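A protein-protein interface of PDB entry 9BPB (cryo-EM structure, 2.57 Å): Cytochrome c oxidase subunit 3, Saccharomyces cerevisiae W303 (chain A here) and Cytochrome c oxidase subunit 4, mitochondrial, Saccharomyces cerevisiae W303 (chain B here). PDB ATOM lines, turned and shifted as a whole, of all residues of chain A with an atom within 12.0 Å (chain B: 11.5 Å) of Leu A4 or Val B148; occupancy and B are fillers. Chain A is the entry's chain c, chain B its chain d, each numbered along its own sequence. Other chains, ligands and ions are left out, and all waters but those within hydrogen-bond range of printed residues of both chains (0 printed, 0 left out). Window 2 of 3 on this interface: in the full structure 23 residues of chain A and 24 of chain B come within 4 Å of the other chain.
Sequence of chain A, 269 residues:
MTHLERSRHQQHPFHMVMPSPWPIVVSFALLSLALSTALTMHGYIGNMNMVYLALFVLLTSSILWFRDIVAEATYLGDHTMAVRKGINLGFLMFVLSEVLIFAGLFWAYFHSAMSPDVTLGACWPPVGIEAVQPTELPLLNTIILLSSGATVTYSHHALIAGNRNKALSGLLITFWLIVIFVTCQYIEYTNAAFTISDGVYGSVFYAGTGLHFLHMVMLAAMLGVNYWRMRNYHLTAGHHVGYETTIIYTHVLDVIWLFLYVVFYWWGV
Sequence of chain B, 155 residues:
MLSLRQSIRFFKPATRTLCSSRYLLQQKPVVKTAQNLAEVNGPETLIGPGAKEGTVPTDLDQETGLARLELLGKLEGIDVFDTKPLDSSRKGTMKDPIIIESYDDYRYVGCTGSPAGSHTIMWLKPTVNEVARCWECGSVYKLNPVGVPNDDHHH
ND1 of His A3 sits at hydrogen-bond distance from OH of Tyr B103 (3.4 Å).
The side-chain carboxylate (OE2) of Glu A5 is in hydrogen-bond range of the backbone NH (N) of Gly B42, at 2.7 Å.
O of Leu A4 lies within hydrogen-bond range of OG of Ser A7 (2.8 Å).
The backbone carbonyl oxygen of Gln A10 is in hydrogen-bond range of the guanidinium group of Arg A6, 2.7 Å away.
O of Arg A6 lies within hydrogen-bond range of NE2 of Gln A11, 3.2 Å away.
The backbone carbonyl oxygen of His A9 lies within hydrogen-bond range of the side-chain amide nitrogen of Gln A11 (3.1 Å).
The backbone carbonyl oxygen (O) of Glu B39 lies close to the side-chain amide oxygen (OD1) of Asn B41, at 3.2 Å.
The backbone NH (N) of Val B146 lies within hydrogen-bond range of the backbone carbonyl oxygen (O) of Ser B102 (3.3 Å).
Among the printed residues, merely in contact across the chains: His A3 with Glu B101 (3.6 Å), His A3 with Val B146 (3.7 Å), Leu A4 with Val B148 (3.5 Å), Glu A5 with Val B40 (3.7 Å), Glu A5 with Asn B41 (3.6 Å), Arg A6 with Tyr B103 (3.3 Å), His A9 with Gly B42 (3.7 Å), His A9 with Leu B69 (3.5 Å) and Gln A11 with Tyr B103 (3.2 Å).
Thr A2 touches none of the printed residues of chain B.
His A3 touches just these residues of chain B: Glu B101, Tyr B103 and Val B146.
Of the printed residues of chain B, Leu A4 touches Val B148.
Glu A5 touches three residues of chain B.
Printed residues of chain B within 4 Å of His A9: Gly B42 (3.7 Å) and Leu B69 (3.5 Å).
Of the printed residues of chain B, Gln A11 touches Tyr B103 (3.2 Å).
Of the printed residues of chain A, Glu B101 touches His A3 (3.6 Å).
Of the printed residues of chain A, Tyr B103 touches His A3 (3.4 Å), Arg A6 (3.3 Å) and Gln A11 (3.2 Å).
Of the printed residues of chain A, Val B146 touches His A3.
Printed residues of chain A within 4 Å of Val B148: Leu A4 (3.5 Å).
The nearest residue of chain B that does not touch Leu A4 is Tyr B103 (6.1 Å).
Of the 20 printed residues of chain B, 8 touch a printed residue of chain A.
Among the printed residues, 11 pairs touch across the chains.
Among the printed residues, no Asp or Glu carboxylate lies within 4 Å of a Lys or Arg side-chain nitrogen of the other chain.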
ATOM      1  N   MET A   1     -10.096   5.707  17.391  1.00  0.00           N
ATOM      2  CA  MET A   1      -9.842   5.001  16.141  1.00  0.00           C
ATOM      3  C   MET A   1     -10.172   3.517  16.273  1.00  0.00           C
ATOM      4  O   MET A   1      -9.708   2.847  17.194  1.00  0.00           O
ATOM      5  CB  MET A   1      -8.387   5.181  15.711  1.00  0.00           C
ATOM      6  CG  MET A   1      -8.150   4.969  14.227  1.00  0.00           C
ATOM      7  SD  MET A   1      -6.431   5.223  13.761  1.00  0.00           S
ATOM      8  CE  MET A   1      -6.618   5.889  12.114  1.00  0.00           C
ATOM      9  N   THR A   2     -11.004   3.020  15.355  1.00  0.00           N
ATOM     10  CA  THR A   2     -11.443   1.608  15.405  1.00  0.00           C
ATOM     11  C   THR A   2     -10.279   0.692  15.068  1.00  0.00           C
ATOM     12  O   THR A   2      -9.392   1.131  14.330  1.00  0.00           O
ATOM     13  CB  THR A   2     -12.559   1.334  14.396  1.00  0.00           C
ATOM     14  OG1 THR A   2     -13.546   2.354  14.541  1.00  0.00           O
ATOM     15  CG2 THR A   2     -13.209  -0.020  14.567  1.00  0.00           C
ATOM     16  N   HIS A   3     -10.270  -0.508  15.626  1.00  0.00           N
ATOM     17  CA  HIS A   3      -9.273  -1.521  15.294  1.00  0.00           C
ATOM     18  C   HIS A   3      -9.266  -1.829  13.802  1.00  0.00           C
ATOM     19  O   HIS A   3      -8.205  -2.101  13.229  1.00  0.00           O
ATOM     20  CB  HIS A   3      -9.531  -2.801  16.088  1.00  0.00           C
ATOM     21  CG  HIS A   3      -8.690  -2.937  17.319  1.00  0.00           C
ATOM     22  ND1 HIS A   3      -7.314  -2.974  17.281  1.00  0.00           N
ATOM     23  CD2 HIS A   3      -9.033  -3.060  18.624  1.00  0.00           C
ATOM     24  CE1 HIS A   3      -6.844  -3.103  18.509  1.00  0.00           C
ATOM     25  NE2 HIS A   3      -7.866  -3.158  19.343  1.00  0.00           N
ATOM     26  N   LEU A   4     -10.435  -1.772  13.156  1.00  0.00           N
ATOM     27  CA  LEU A   4     -10.517  -2.063  11.699  1.00  0.00           C
ATOM     28  C   LEU A   4      -9.820  -0.955  10.905  1.00  0.00           C
ATOM     29  O   LEU A   4      -9.170  -1.281   9.903  1.00  0.00           O
ATOM     30  CB  LEU A   4     -11.979  -2.192  11.272  1.00  0.00           C
ATOM     31  CG  LEU A   4     -12.199  -2.561   9.809  1.00  0.00           C
ATOM     32  CD1 LEU A   4     -12.110  -4.063   9.616  1.00  0.00           C
ATOM     33  CD2 LEU A   4     -13.533  -2.034   9.312  1.00  0.00           C
ATOM     34  N   GLU A   5      -9.959   0.304  11.327  1.00  0.00           N
ATOM     35  CA  GLU A   5      -9.360   1.403  10.578  1.00  0.00           C
ATOM     36  C   GLU A   5      -7.841   1.396  10.689  1.00  0.00           C
ATOM     37  O   GLU A   5      -7.140   1.655   9.705  1.00  0.00           O
ATOM     38  CB  GLU A   5      -9.926   2.735  11.067  1.00  0.00           C
ATOM     39  CG  GLU A   5      -9.347   3.955  10.373  1.00  0.00           C
ATOM     40  CD  GLU A   5      -9.721   4.026   8.906  1.00  0.00           C
ATOM     41  OE1 GLU A   5     -10.774   3.470   8.530  1.00  0.00           O
ATOM     42  OE2 GLU A   5      -8.961   4.641   8.130  1.00  0.00           O
ATOM     43  N   ARG A   6      -7.315   1.109  11.883  1.00  0.00           N
ATOM     44  CA  ARG A   6      -5.871   1.159  12.087  1.00  0.00           C
ATOM     45  C   ARG A   6      -5.140   0.132  11.233  1.00  0.00           C
ATOM     46  O   ARG A   6      -3.989   0.359  10.842  1.00  0.00           O
ATOM     47  CB  ARG A   6      -5.547   0.950  13.565  1.00  0.00           C
ATOM     48  CG  ARG A   6      -4.084   1.164  13.916  1.00  0.00           C
ATOM     49  CD  ARG A   6      -3.573   2.470  13.347  1.00  0.00           C
ATOM     50  NE  ARG A   6      -2.152   2.658  13.603  1.00  0.00           N
ATOM     51  CZ  ARG A   6      -1.194   2.380  12.730  1.00  0.00           C
ATOM     52  NH1 ARG A   6      -1.472   1.876  11.538  1.00  0.00           N
ATOM     53  NH2 ARG A   6       0.071   2.610  13.059  1.00  0.00           N
ATOM     54  N   SER A   7      -5.784  -0.990  10.925  1.00  0.00           N
ATOM     55  CA  SER A   7      -5.169  -2.041  10.124  1.00  0.00           C
ATOM     56  C   SER A   7      -5.104  -1.693   8.645  1.00  0.00           C
ATOM     57  O   SER A   7      -4.554  -2.472   7.862  1.00  0.00           O
ATOM     58  CB  SER A   7      -5.931  -3.353  10.311  1.00  0.00           C
ATOM     59  OG  SER A   7      -7.224  -3.274   9.737  1.00  0.00           O
ATOM     60  N   ARG A   8      -5.654  -0.549   8.250  1.00  0.00           N
ATOM     61  CA  ARG A   8      -5.667  -0.090   6.869  1.00  0.00           C
ATOM     62  C   ARG A   8      -4.593   0.980   6.678  1.00  0.00           C
ATOM     63  O   ARG A   8      -4.738   1.922   5.900  1.00  0.00           O
ATOM     64  CB  ARG A   8      -7.063   0.414   6.503  1.00  0.00           C
ATOM     65  CG  ARG A   8      -7.297   0.804   5.052  1.00  0.00           C
ATOM     66  CD  ARG A   8      -8.720   0.474   4.643  1.00  0.00           C
ATOM     67  NE  ARG A   8      -9.668   0.773   5.708  1.00  0.00           N
ATOM     68  CZ  ARG A   8     -10.619   1.694   5.630  1.00  0.00           C
ATOM     69  NH1 ARG A   8     -10.782   2.429   4.543  1.00  0.00           N
ATOM     70  NH2 ARG A   8     -11.428   1.879   6.669  1.00  0.00           N
ATOM     71  N   HIS A   9      -3.486   0.830   7.405  1.00  0.00           N
ATOM     72  CA  HIS A   9      -2.397   1.796   7.408  1.00  0.00           C
ATOM     73  C   HIS A   9      -1.116   1.069   7.789  1.00  0.00           C
ATOM     74  O   HIS A   9      -1.146  -0.062   8.280  1.00  0.00           O
ATOM     75  CB  HIS A   9      -2.659   2.949   8.386  1.00  0.00           C
ATOM     76  CG  HIS A   9      -3.795   3.842   7.989  1.00  0.00           C
ATOM     77  ND1 HIS A   9      -3.675   4.814   7.019  1.00  0.00           N
ATOM     78  CD2 HIS A   9      -5.074   3.905   8.428  1.00  0.00           C
ATOM     79  CE1 HIS A   9      -4.830   5.440   6.879  1.00  0.00           C
ATOM     80  NE2 HIS A   9      -5.696   4.907   7.723  1.00  0.00           N
ATOM     81  N   GLN A  10       0.019   1.723   7.538  1.00  0.00           N
ATOM     82  CA  GLN A  10       1.326   1.110   7.887  1.00  0.00           C
ATOM     83  C   GLN A  10       1.419   1.012   9.405  1.00  0.00           C
ATOM     84  O   GLN A  10       0.861   1.880  10.087  1.00  0.00           O
ATOM     85  CB  GLN A  10       2.513   1.906   7.344  1.00  0.00           C
ATOM     86  CG  GLN A  10       3.064   1.379   6.031  1.00  0.00           C
ATOM     87  CD  GLN A  10       4.340   2.088   5.657  1.00  0.00           C
ATOM     88  OE1 GLN A  10       4.468   2.656   4.575  1.00  0.00           O
ATOM     89  NE2 GLN A  10       5.309   2.050   6.556  1.00  0.00           N
ATOM     90  N   GLN A  11       2.095  -0.011   9.906  1.00  0.00           N
ATOM     91  CA  GLN A  11       2.245  -0.225  11.368  1.00  0.00           C
ATOM     92  C   GLN A  11       3.602   0.328  11.798  1.00  0.00           C
ATOM     93  O   GLN A  11       3.884   0.324  13.005  1.00  0.00           O
ATOM     94  CB  GLN A  11       2.113  -1.705  11.725  1.00  0.00           C
ATOM     95  CG  GLN A  11       0.895  -2.396  11.138  1.00  0.00           C
ATOM     96  CD  GLN A  11      -0.380  -1.928  11.792  1.00  0.00           C
ATOM     97  OE1 GLN A  11      -0.510  -1.951  13.012  1.00  0.00           O
ATOM     98  NE2 GLN A  11      -1.325  -1.485  10.982  1.00  0.00           N
ATOM     99  N   LEU B  37      -8.741  12.439  14.586  1.00  0.00           N
ATOM    100  CA  LEU B  37      -8.214  11.092  14.392  1.00  0.00           C
ATOM    101  C   LEU B  37      -9.328  10.058  14.286  1.00  0.00           C
ATOM    102  O   LEU B  37      -9.108   8.965  13.758  1.00  0.00           O
ATOM    103  CB  LEU B  37      -7.264  10.734  15.532  1.00  0.00           C
ATOM    104  CG  LEU B  37      -6.302   9.574  15.284  1.00  0.00           C
ATOM    105  CD1 LEU B  37      -5.317   9.926  14.188  1.00  0.00           C
ATOM    106  CD2 LEU B  37      -5.573   9.218  16.561  1.00  0.00           C
ATOM    107  N   ALA B  38     -10.526  10.385  14.776  1.00  0.00           N
ATOM    108  CA  ALA B  38     -11.636   9.443  14.731  1.00  0.00           C
ATOM    109  C   ALA B  38     -12.442   9.547  13.445  1.00  0.00           C
ATOM    110  O   ALA B  38     -13.384   8.771  13.256  1.00  0.00           O
ATOM    111  CB  ALA B  38     -12.555   9.657  15.933  1.00  0.00           C
ATOM    112  N   GLU B  39     -12.246  10.631  12.706  1.00  0.00           N
ATOM    113  CA  GLU B  39     -13.084  10.808  11.499  1.00  0.00           C
ATOM    114  C   GLU B  39     -12.259  10.249  10.351  1.00  0.00           C
ATOM    115  O   GLU B  39     -12.755  10.208   9.205  1.00  0.00           O
ATOM    116  CB  GLU B  39     -13.431  12.280  11.284  1.00  0.00           C
ATOM    117  CG  GLU B  39     -13.837  12.992  12.560  1.00  0.00           C
ATOM    118  CD  GLU B  39     -14.779  14.167  12.367  1.00  0.00           C
ATOM    119  OE1 GLU B  39     -15.257  14.363  11.233  1.00  0.00           O
ATOM    120  OE2 GLU B  39     -15.017  14.895  13.350  1.00  0.00           O
ATOM    121  N   VAL B  40     -11.050   9.795  10.679  1.00  0.00           N
ATOM    122  CA  VAL B  40     -10.158   9.353   9.576  1.00  0.00           C
ATOM    123  C   VAL B  40     -10.860   8.193   8.883  1.00  0.00           C
ATOM    124  O   VAL B  40     -11.379   7.302   9.588  1.00  0.00           O
ATOM    125  CB  VAL B  40      -8.765   8.946  10.095  1.00  0.00           C
ATOM    126  CG1 VAL B  40      -7.917   8.308   9.004  1.00  0.00           C
ATOM    127  CG2 VAL B  40      -8.032  10.122  10.723  1.00  0.00           C
ATOM    128  N   ASN B  41     -10.905   8.238   7.554  1.00  0.00           N
ATOM    129  CA  ASN B  41     -11.458   7.103   6.781  1.00  0.00           C
ATOM    130  C   ASN B  41     -10.388   6.871   5.729  1.00  0.00           C
ATOM    131  O   ASN B  41     -10.657   7.107   4.536  1.00  0.00           O
ATOM    132  CB  ASN B  41     -12.840   7.391   6.198  1.00  0.00           C
ATOM    133  CG  ASN B  41     -13.965   6.963   7.116  1.00  0.00           C
ATOM    134  OD1 ASN B  41     -14.078   7.451   8.238  1.00  0.00           O
ATOM    135  ND2 ASN B  41     -14.800   6.050   6.649  1.00  0.00           N
ATOM    136  N   GLY B  42      -9.218   6.435   6.190  1.00  0.00           N
ATOM    137  CA  GLY B  42      -8.093   6.224   5.267  1.00  0.00           C
ATOM    138  C   GLY B  42      -7.500   7.516   4.725  1.00  0.00           C
ATOM    139  O   GLY B  42      -7.428   8.513   5.467  1.00  0.00           O
ATOM    140  N   PRO B  43      -7.052   7.522   3.459  1.00  0.00           N
ATOM    141  CA  PRO B  43      -6.384   8.689   2.842  1.00  0.00           C
ATOM    142  C   PRO B  43      -7.185   9.918   2.372  1.00  0.00           C
ATOM    143  O   PRO B  43      -6.701  11.014   2.580  1.00  0.00           O
ATOM    144  CB  PRO B  43      -5.734   8.077   1.587  1.00  0.00           C
ATOM    145  CG  PRO B  43      -6.604   6.889   1.261  1.00  0.00           C
ATOM    146  CD  PRO B  43      -6.977   6.328   2.616  1.00  0.00           C
ATOM    147  N   LEU B  69      -1.507  11.679   9.116  1.00  0.00           N
ATOM    148  CA  LEU B  69      -2.123  10.871  10.162  1.00  0.00           C
ATOM    149  C   LEU B  69      -1.317  10.947  11.451  1.00  0.00           C
ATOM    150  O   LEU B  69      -1.888  11.003  12.547  1.00  0.00           O
ATOM    151  CB  LEU B  69      -2.263   9.425   9.692  1.00  0.00           C
ATOM    152  CG  LEU B  69      -3.218   8.518  10.468  1.00  0.00           C
ATOM    153  CD1 LEU B  69      -3.892   7.544   9.525  1.00  0.00           C
ATOM    154  CD2 LEU B  69      -2.491   7.762  11.563  1.00  0.00           C
ATOM    155  N   GLU B 101      -0.198  -8.378  22.347  1.00  0.00           N
ATOM    156  CA  GLU B 101      -1.208  -7.976  21.377  1.00  0.00           C
ATOM    157  C   GLU B 101      -0.547  -7.668  20.040  1.00  0.00           C
ATOM    158  O   GLU B 101       0.395  -6.873  19.974  1.00  0.00           O
ATOM    159  CB  GLU B 101      -1.979  -6.761  21.891  1.00  0.00           C
ATOM    160  CG  GLU B 101      -2.685  -5.955  20.825  1.00  0.00           C
ATOM    161  CD  GLU B 101      -3.525  -4.840  21.414  1.00  0.00           C
ATOM    162  OE1 GLU B 101      -3.553  -4.712  22.656  1.00  0.00           O
ATOM    163  OE2 GLU B 101      -4.156  -4.092  20.638  1.00  0.00           O
ATOM    164  N   SER B 102      -1.043  -8.299  18.976  1.00  0.00           N
ATOM    165  CA  SER B 102      -0.457  -8.154  17.652  1.00  0.00           C
ATOM    166  C   SER B 102      -1.557  -8.047  16.605  1.00  0.00           C
ATOM    167  O   SER B 102      -2.683  -8.508  16.805  1.00  0.00           O
ATOM    168  CB  SER B 102       0.473  -9.326  17.316  1.00  0.00           C
ATOM    169  OG  SER B 102       0.988  -9.208  16.003  1.00  0.00           O
ATOM    170  N   TYR B 103      -1.210  -7.426  15.481  1.00  0.00           N
ATOM    171  CA  TYR B 103      -2.107  -7.287  14.342  1.00  0.00           C
ATOM    172  C   TYR B 103      -2.012  -8.458  13.374  1.00  0.00           C
ATOM    173  O   TYR B 103      -2.749  -8.487  12.382  1.00  0.00           O
ATOM    174  CB  TYR B 103      -1.816  -5.978  13.599  1.00  0.00           C
ATOM    175  CG  TYR B 103      -2.611  -4.801  14.114  1.00  0.00           C
ATOM    176  CD1 TYR B 103      -3.927  -4.602  13.722  1.00  0.00           C
ATOM    177  CD2 TYR B 103      -2.045  -3.893  14.998  1.00  0.00           C
ATOM    178  CE1 TYR B 103      -4.655  -3.532  14.193  1.00  0.00           C
ATOM    179  CE2 TYR B 103      -2.766  -2.820  15.474  1.00  0.00           C
ATOM    180  CZ  TYR B 103      -4.070  -2.643  15.069  1.00  0.00           C
ATOM    181  OH  TYR B 103      -4.794  -1.575  15.545  1.00  0.00           O
ATOM    182  N   ASP B 104      -1.133  -9.415  13.639  1.00  0.00           N
ATOM    183  CA  ASP B 104      -0.885 -10.554  12.770  1.00  0.00           C
ATOM    184  C   ASP B 104      -1.229 -11.841  13.515  1.00  0.00           C
ATOM    185  O   ASP B 104      -1.802 -11.820  14.607  1.00  0.00           O
ATOM    186  CB  ASP B 104       0.569 -10.563  12.303  1.00  0.00           C
ATOM    187  CG  ASP B 104       0.951  -9.298  11.582  1.00  0.00           C
ATOM    188  OD1 ASP B 104       0.059  -8.651  10.998  1.00  0.00           O
ATOM    189  OD2 ASP B 104       2.148  -8.948  11.610  1.00  0.00           O
ATOM    190  N   ASP B 105      -0.874 -12.967  12.908  1.00  0.00           N
ATOM    191  CA  ASP B 105      -1.029 -14.268  13.536  1.00  0.00           C
ATOM    192  C   ASP B 105       0.212 -14.695  14.309  1.00  0.00           C
ATOM    193  O   ASP B 105       0.299 -15.854  14.726  1.00  0.00           O
ATOM    194  CB  ASP B 105      -1.376 -15.322  12.481  1.00  0.00           C
ATOM    195  CG  ASP B 105      -2.857 -15.352  12.150  1.00  0.00           C
ATOM    196  OD1 ASP B 105      -3.564 -14.375  12.479  1.00  0.00           O
ATOM    197  OD2 ASP B 105      -3.314 -16.351  11.559  1.00  0.00           O
ATOM    198  N   TYR B 106       1.169 -13.791  14.509  1.00  0.00           N
ATOM    199  CA  TYR B 106       2.371 -14.100  15.271  1.00  0.00           C
ATOM    200  C   TYR B 106       3.031 -12.798  15.696  1.00  0.00           C
ATOM    201  O   TYR B 106       2.642 -11.709  15.268  1.00  0.00           O
ATOM    202  CB  TYR B 106       3.348 -14.961  14.464  1.00  0.00           C
ATOM    203  CG  TYR B 106       3.964 -14.246  13.281  1.00  0.00           C
ATOM    204  CD1 TYR B 106       3.277 -14.126  12.082  1.00  0.00           C
ATOM    205  CD2 TYR B 106       5.231 -13.687  13.368  1.00  0.00           C
ATOM    206  CE1 TYR B 106       3.836 -13.473  11.004  1.00  0.00           C
ATOM    207  CE2 TYR B 106       5.798 -13.033  12.297  1.00  0.00           C
ATOM    208  CZ  TYR B 106       5.096 -12.927  11.116  1.00  0.00           C
ATOM    209  OH  TYR B 106       5.659 -12.274  10.045  1.00  0.00           O
ATOM    210  N   VAL B 128      -0.859 -17.796  17.071  1.00  0.00           N
ATOM    211  CA  VAL B 128      -2.204 -18.265  17.356  1.00  0.00           C
ATOM    212  C   VAL B 128      -2.163 -19.773  17.558  1.00  0.00           C
ATOM    213  O   VAL B 128      -1.497 -20.499  16.808  1.00  0.00           O
ATOM    214  CB  VAL B 128      -3.163 -17.875  16.218  1.00  0.00           C
ATOM    215  CG1 VAL B 128      -4.579 -18.311  16.544  1.00  0.00           C
ATOM    216  CG2 VAL B 128      -3.107 -16.377  15.973  1.00  0.00           C
ATOM    217  N   ASN B 144      -2.659 -12.148  21.486  1.00  0.00           N
ATOM    218  CA  ASN B 144      -4.011 -11.611  21.387  1.00  0.00           C
ATOM    219  C   ASN B 144      -4.219 -11.080  19.977  1.00  0.00           C
ATOM    220  O   ASN B 144      -3.760  -9.970  19.665  1.00  0.00           O
ATOM    221  CB  ASN B 144      -4.234 -10.505  22.419  1.00  0.00           C
ATOM    222  CG  ASN B 144      -5.593  -9.851  22.286  1.00  0.00           C
ATOM    223  OD1 ASN B 144      -5.719  -8.631  22.390  1.00  0.00           O
ATOM    224  ND2 ASN B 144      -6.620 -10.658  22.061  1.00  0.00           N
ATOM    225  N   PRO B 145      -4.889 -11.826  19.099  1.00  0.00           N
ATOM    226  CA  PRO B 145      -5.010 -11.466  17.667  1.00  0.00           C
ATOM    227  C   PRO B 145      -6.119 -10.469  17.331  1.00  0.00           C
ATOM    228  O   PRO B 145      -7.235 -10.816  16.940  1.00  0.00           O
ATOM    229  CB  PRO B 145      -5.259 -12.824  17.009  1.00  0.00           C
ATOM    230  CG  PRO B 145      -6.001 -13.604  18.051  1.00  0.00           C
ATOM    231  CD  PRO B 145      -5.586 -13.086  19.407  1.00  0.00           C
ATOM    232  N   VAL B 146      -5.811  -9.185  17.486  1.00  0.00           N
ATOM    233  CA  VAL B 146      -6.713  -8.108  17.097  1.00  0.00           C
ATOM    234  C   VAL B 146      -6.280  -7.584  15.735  1.00  0.00           C
ATOM    235  O   VAL B 146      -5.102  -7.277  15.522  1.00  0.00           O
ATOM    236  CB  VAL B 146      -6.737  -6.985  18.149  1.00  0.00           C
ATOM    237  CG1 VAL B 146      -7.382  -7.481  19.430  1.00  0.00           C
ATOM    238  CG2 VAL B 146      -5.335  -6.474  18.432  1.00  0.00           C
ATOM    239  N   GLY B 147      -7.223  -7.510  14.800  1.00  0.00           N
ATOM    240  CA  GLY B 147      -6.909  -7.052  13.461  1.00  0.00           C
ATOM    241  C   GLY B 147      -7.680  -7.777  12.376  1.00  0.00           C
ATOM    242  O   GLY B 147      -8.399  -8.743  12.657  1.00  0.00           O
ATOM    243  N   VAL B 148      -7.529  -7.316  11.136  1.00  0.00           N
ATOM    244  CA  VAL B 148      -8.243  -7.863   9.982  1.00  0.00           C
ATOM    245  C   VAL B 148      -9.749  -7.845  10.219  1.00  0.00           C
ATOM    246  O   VAL B 148     -10.309  -6.832  10.637  1.00  0.00           O
ATOM    247  CB  VAL B 148      -7.763  -9.288   9.643  1.00  0.00           C
ATOM    248  CG1 VAL B 148      -8.638  -9.898   8.555  1.00  0.00           C
